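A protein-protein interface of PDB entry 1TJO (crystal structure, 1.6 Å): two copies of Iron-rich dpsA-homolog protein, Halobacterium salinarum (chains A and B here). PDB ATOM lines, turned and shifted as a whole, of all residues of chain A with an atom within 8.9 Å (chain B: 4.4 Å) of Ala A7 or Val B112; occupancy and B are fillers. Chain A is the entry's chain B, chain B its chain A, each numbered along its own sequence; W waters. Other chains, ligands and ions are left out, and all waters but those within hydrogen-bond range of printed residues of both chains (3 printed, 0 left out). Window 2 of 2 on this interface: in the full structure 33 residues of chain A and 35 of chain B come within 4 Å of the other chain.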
ATOM      1  N   ALA A   7     -31.331  18.950   7.835  1.00  0.00           N
ATOM      2  CA  ALA A   7     -30.233  19.609   7.067  1.00  0.00           C
ATOM      3  C   ALA A   7     -30.538  21.057   6.773  1.00  0.00           C
ATOM      4  O   ALA A   7     -31.670  21.409   6.451  1.00  0.00           O
ATOM      5  CB  ALA A   7     -29.993  18.858   5.768  1.00  0.00           C
ATOM      6  N   ARG A   8     -29.513  21.906   6.856  1.00  0.00           N
ATOM      7  CA  ARG A   8     -29.631  23.299   6.461  1.00  0.00           C
ATOM      8  C   ARG A   8     -29.730  23.515   4.988  1.00  0.00           C
ATOM      9  O   ARG A   8     -30.373  24.456   4.545  1.00  0.00           O
ATOM     10  CB  ARG A   8     -28.376  24.105   6.904  1.00  0.00           C
ATOM     11  CG  ARG A   8     -28.538  24.717   8.188  1.00  0.00           C
ATOM     12  CD  ARG A   8     -27.368  25.560   8.607  1.00  0.00           C
ATOM     13  NE  ARG A   8     -27.466  26.959   8.172  1.00  0.00           N
ATOM     14  CZ  ARG A   8     -28.437  27.799   8.556  1.00  0.00           C
ATOM     15  NH1 ARG A   8     -29.384  27.413   9.385  1.00  0.00           N
ATOM     16  NH2 ARG A   8     -28.434  29.059   8.138  1.00  0.00           N
ATOM     17  N   ALA A   9     -28.998  22.722   4.215  1.00  0.00           N
ATOM     18  CA  ALA A   9     -29.032  22.811   2.767  1.00  0.00           C
ATOM     19  C   ALA A   9     -28.745  21.461   2.219  1.00  0.00           C
ATOM     20  O   ALA A   9     -28.045  20.685   2.805  1.00  0.00           O
ATOM     21  CB  ALA A   9     -28.040  23.794   2.209  1.00  0.00           C
ATOM     22  N   THR A  10     -29.344  21.189   1.077  1.00  0.00           N
ATOM     23  CA  THR A  10     -29.284  19.892   0.504  1.00  0.00           C
ATOM     24  C   THR A  10     -28.290  20.015  -0.660  1.00  0.00           C
ATOM     25  O   THR A  10     -28.298  21.003  -1.330  1.00  0.00           O
ATOM     26  CB  THR A  10     -30.747  19.570   0.123  1.00  0.00           C
ATOM     27  OG1 THR A  10     -31.255  18.586   1.020  1.00  0.00           O
ATOM     28  CG2 THR A  10     -30.875  19.019  -1.145  1.00  0.00           C
ATOM     29  N   ALA A  11     -27.367  19.056  -0.809  1.00  0.00           N
ATOM     30  CA  ALA A  11     -26.440  19.015  -1.932  1.00  0.00           C
ATOM     31  C   ALA A  11     -27.214  19.081  -3.210  1.00  0.00           C
ATOM     32  O   ALA A  11     -28.105  18.232  -3.457  1.00  0.00           O
ATOM     33  CB  ALA A  11     -25.603  17.749  -1.918  1.00  0.00           C
ATOM     34  N   GLY A  12     -26.873  20.021  -4.063  1.00  0.00           N
ATOM     35  CA  GLY A  12     -27.663  20.210  -5.283  1.00  0.00           C
ATOM     36  C   GLY A  12     -28.706  21.321  -5.258  1.00  0.00           C
ATOM     37  O   GLY A  12     -29.165  21.755  -6.308  1.00  0.00           O
ATOM     38  N   GLU A  13     -29.108  21.805  -4.097  1.00  0.00           N
ATOM     39  CA  GLU A  13     -29.933  23.015  -4.042  1.00  0.00           C
ATOM     40  C   GLU A  13     -29.070  24.217  -4.346  1.00  0.00           C
ATOM     41  O   GLU A  13     -27.910  24.268  -3.967  1.00  0.00           O
ATOM     42  CB  GLU A  13     -30.553  23.241  -2.655  1.00  0.00           C
ATOM     43  CG  GLU A  13     -31.671  22.296  -2.318  1.00  0.00           C
ATOM     44  CD  GLU A  13     -32.314  22.567  -0.951  1.00  0.00           C
ATOM     45  OE1 GLU A  13     -33.532  22.285  -0.843  1.00  0.00           O
ATOM     46  OE2 GLU A  13     -31.613  23.031   0.011  1.00  0.00           O
ATOM     47  N   GLN A  86     -20.720  28.617  -2.483  1.00  0.00           N
ATOM     48  CA  GLN A  86     -21.448  28.833  -1.268  1.00  0.00           C
ATOM     49  C   GLN A  86     -22.090  30.238  -1.280  1.00  0.00           C
ATOM     50  O   GLN A  86     -23.261  30.414  -0.892  1.00  0.00           O
ATOM     51  CB  GLN A  86     -20.517  28.682  -0.100  1.00  0.00           C
ATOM     52  CG  GLN A  86     -21.180  28.297   1.108  1.00  0.00           C
ATOM     53  CD  GLN A  86     -21.900  29.422   1.706  1.00  0.00           C
ATOM     54  OE1 GLN A  86     -22.996  29.252   2.248  1.00  0.00           O
ATOM     55  NE2 GLN A  86     -21.310  30.575   1.641  1.00  0.00           N
ATOM     56  N   GLY A  89     -25.328  30.600  -3.085  1.00  0.00           N
ATOM     57  CA  GLY A  89     -26.360  29.806  -2.518  1.00  0.00           C
ATOM     58  C   GLY A  89     -26.349  28.328  -2.878  1.00  0.00           C
ATOM     59  O   GLY A  89     -27.362  27.676  -2.690  1.00  0.00           O
ATOM     60  N   GLY A  90     -25.223  27.796  -3.350  1.00  0.00           N
ATOM     61  CA  GLY A  90     -25.075  26.373  -3.521  1.00  0.00           C
ATOM     62  C   GLY A  90     -24.217  25.691  -2.486  1.00  0.00           C
ATOM     63  O   GLY A  90     -23.799  26.286  -1.478  1.00  0.00           O
ATOM     64  N   VAL A  91     -24.016  24.401  -2.699  1.00  0.00           N
ATOM     65  CA  VAL A  91     -23.270  23.547  -1.798  1.00  0.00           C
ATOM     66  C   VAL A  91     -22.028  23.056  -2.549  1.00  0.00           C
ATOM     67  O   VAL A  91     -22.147  22.291  -3.537  1.00  0.00           O
ATOM     68  CB  VAL A  91     -24.127  22.356  -1.342  1.00  0.00           C
ATOM     69  CG1 VAL A  91     -23.337  21.442  -0.474  1.00  0.00           C
ATOM     70  CG2 VAL A  91     -25.326  22.856  -0.555  1.00  0.00           C
ATOM     71  N   PRO A  92     -20.850  23.411  -2.074  1.00  0.00           N
ATOM     72  CA  PRO A  92     -19.646  22.950  -2.756  1.00  0.00           C
ATOM     73  C   PRO A  92     -19.430  21.432  -2.471  1.00  0.00           C
ATOM     74  O   PRO A  92     -19.628  20.971  -1.353  1.00  0.00           O
ATOM     75  CB  PRO A  92     -18.544  23.852  -2.183  1.00  0.00           C
ATOM     76  CG  PRO A  92     -19.075  24.291  -0.856  1.00  0.00           C
ATOM     77  CD  PRO A  92     -20.565  24.329  -0.935  1.00  0.00           C
ATOM     78  N   HIS A  93     -18.954  20.691  -3.476  1.00  0.00           N
ATOM     79  CA  HIS A  93     -18.519  19.313  -3.288  1.00  0.00           C
ATOM     80  C   HIS A  93     -17.444  19.278  -2.205  1.00  0.00           C
ATOM     81  O   HIS A  93     -16.521  20.107  -2.230  1.00  0.00           O
ATOM     82  CB  HIS A  93     -17.906  18.783  -4.591  1.00  0.00           C
ATOM     83  CG  HIS A  93     -18.856  18.726  -5.749  1.00  0.00           C
ATOM     84  ND1 HIS A  93     -20.166  18.311  -5.619  1.00  0.00           N
ATOM     85  CD2 HIS A  93     -18.677  19.026  -7.052  1.00  0.00           C
ATOM     86  CE1 HIS A  93     -20.750  18.348  -6.808  1.00  0.00           C
ATOM     87  NE2 HIS A  93     -19.879  18.804  -7.690  1.00  0.00           N
ATOM     88  N   ALA A  94     -17.522  18.342  -1.255  1.00  0.00           N
ATOM     89  CA  ALA A  94     -16.696  18.410  -0.076  1.00  0.00           C
ATOM     90  C   ALA A  94     -15.885  17.114   0.201  1.00  0.00           C
ATOM     91  O   ALA A  94     -14.677  17.153   0.406  1.00  0.00           O
ATOM     92  CB  ALA A  94     -17.542  18.782   1.105  1.00  0.00           C
ATOM     93  N   ASN B  54     -19.073  26.612   4.671  1.00  0.00           N
ATOM     94  CA  ASN B  54     -20.513  26.629   4.782  1.00  0.00           C
ATOM     95  C   ASN B  54     -21.002  27.314   6.065  1.00  0.00           C
ATOM     96  O   ASN B  54     -22.177  27.643   6.157  1.00  0.00           O
ATOM     97  CB  ASN B  54     -21.062  25.205   4.714  1.00  0.00           C
ATOM     98  CG  ASN B  54     -21.005  24.611   3.316  1.00  0.00           C
ATOM     99  OD1 ASN B  54     -21.475  25.209   2.379  1.00  0.00           O
ATOM    100  ND2 ASN B  54     -20.415  23.447   3.177  1.00  0.00           N
ATOM    101  N   GLU B 110     -23.100  14.633   1.897  1.00  0.00           N
ATOM    102  CA  GLU B 110     -22.872  15.922   1.208  1.00  0.00           C
ATOM    103  C   GLU B 110     -23.862  17.025   1.525  1.00  0.00           C
ATOM    104  O   GLU B 110     -23.715  18.174   1.028  1.00  0.00           O
ATOM    105  CB  GLU B 110     -22.783  15.690  -0.312  1.00  0.00           C
ATOM    106  CG  GLU B 110     -21.508  14.964  -0.691  1.00  0.00           C
ATOM    107  CD  GLU B 110     -20.278  15.818  -0.428  1.00  0.00           C
ATOM    108  OE1 GLU B 110     -19.409  15.370   0.354  1.00  0.00           O
ATOM    109  OE2 GLU B 110     -20.193  16.912  -1.011  1.00  0.00           O
ATOM    110  N   ASP B 111     -24.870  16.738   2.335  1.00  0.00           N
ATOM    111  CA  ASP B 111     -25.748  17.804   2.763  1.00  0.00           C
ATOM    112  C   ASP B 111     -25.009  18.621   3.812  1.00  0.00           C
ATOM    113  O   ASP B 111     -23.977  18.183   4.340  1.00  0.00           O
ATOM    114  CB  ASP B 111     -27.049  17.274   3.321  1.00  0.00           C
ATOM    115  CG  ASP B 111     -27.912  16.606   2.257  1.00  0.00           C
ATOM    116  OD1 ASP B 111     -27.712  16.844   1.041  1.00  0.00           O
ATOM    117  OD2 ASP B 111     -28.849  15.861   2.580  1.00  0.00           O
ATOM    118  N   VAL B 112     -25.530  19.832   4.040  1.00  0.00           N
ATOM    119  CA  VAL B 112     -24.968  20.782   4.999  1.00  0.00           C
ATOM    120  C   VAL B 112     -25.795  20.810   6.262  1.00  0.00           C
ATOM    121  O   VAL B 112     -26.996  20.998   6.205  1.00  0.00           O
ATOM    122  CB  VAL B 112     -24.913  22.179   4.370  1.00  0.00           C
ATOM    123  CG1 VAL B 112     -24.377  23.228   5.372  1.00  0.00           C
ATOM    124  CG2 VAL B 112     -24.043  22.133   3.165  1.00  0.00           C
ATOM    125  N   TYR B 113     -25.146  20.639   7.403  1.00  0.00           N
ATOM    126  CA  TYR B 113     -25.827  20.612   8.674  1.00  0.00           C
ATOM    127  C   TYR B 113     -25.498  21.852   9.466  1.00  0.00           C
ATOM    128  O   TYR B 113     -24.558  22.609   9.147  1.00  0.00           O
ATOM    129  CB  TYR B 113     -25.443  19.354   9.411  1.00  0.00           C
ATOM    130  CG  TYR B 113     -25.824  18.169   8.563  1.00  0.00           C
ATOM    131  CD1 TYR B 113     -24.911  17.527   7.750  1.00  0.00           C
ATOM    132  CD2 TYR B 113     -27.148  17.745   8.516  1.00  0.00           C
ATOM    133  CE1 TYR B 113     -25.302  16.469   6.904  1.00  0.00           C
ATOM    134  CE2 TYR B 113     -27.529  16.717   7.715  1.00  0.00           C
ATOM    135  CZ  TYR B 113     -26.623  16.079   6.909  1.00  0.00           C
ATOM    136  OH  TYR B 113     -27.055  15.032   6.116  1.00  0.00           O
HETATM  137  O   HOH W   1     -20.201  21.516   1.106  1.00  0.00           O
HETATM  138  O   HOH W   2     -21.720  17.629  -3.222  1.00  0.00           O
HETATM  139  O   HOH W   3     -24.722  26.744   6.552  1.00  0.00           O
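The side-chain carboxylate of Glu B110 sits at hydrogen-bond distance from the backbone NH of Ala A94, at 3.0 Å.
N of Ala A11 is in hydrogen-bond range of OD1 of Asp B111, at 2.9 Å.
The backbone NH of Arg A8 lies within hydrogen-bond range of the backbone carbonyl oxygen of Val B112 (2.8 Å).
The backbone carbonyl oxygen of Ala A9 lies within hydrogen-bond range of the backbone NH of Val B112 (2.9 Å).
The side-chain carboxylate of Glu A13 lies within hydrogen-bond range of the backbone NH of Thr A10, 3.1 Å away.
Val B112 touches Ala A7 (O to C, 3.6 Å).
Ala A7 touches Tyr B113 (CB to CE2, 3.8 Å).
O of Ala A9 touches CB of Asp B111, at 3.6 Å.
OD1 of Asp B111 touches CA of Thr A10, at 3.5 Å.
CB of Ala A11 touches O of Glu B110 (3.5 Å).
OD1 of Asn B54 touches CG of Gln A86, at 3.4 Å.
Val A91 touches Glu B110.
CG1 of Val A91 touches CG2 of Val B112, at 3.8 Å.
Asn B54 touches Pro A92.
His A93 touches Glu B110.
Of the printed residues of chain B, Arg A8 touches Val B112 (2.8 Å).
Glu A13 touches none of the printed residues of chain B.
Gly A90 touches none of the printed residues of chain B.
Of the printed residues of chain A, Glu B110 touches Ala A11 (3.5 Å), Val A91 (3.6 Å), His A93 (3.7 Å) and Ala A94 (3.0 Å).
Of chain A, only Ala A9 (3.6 Å), Thr A10 (3.5 Å) and Ala A11 (2.9 Å) come within 4 Å of Asp B111.
Of the printed residues of chain A, Val B112 touches Ala A7, Arg A8, Ala A9 and Val A91.
The nearest printed residue of chain B that does not touch His A93 is Asn B54 (7.3 Å).
Of the 14 printed residues of chain A, 10 touch a printed residue of chain B.
Along chain A the printed residues that touch a printed residue of chain B span positions 7 to 94.
Hydrophobic or aromatic side chains of chain B that line the printed part of chain A: Val B112 and Tyr B113.
No position is printed for both chains.
Of the 14 pairs that touch across the chains among the printed residues, none has its exchanged pair printed and touching as well.
Water W1 bridges the backbone carbonyl oxygen of Pro A92 and the side-chain amide nitrogen of Asn B54.
Water W3 lies within hydrogen-bond range of O of Asn B54 and NE of Arg A8.
Water W2 bridges the side-chain carboxylate (OE2) of Glu B110 and a ring nitrogen (ND1) of His A93.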
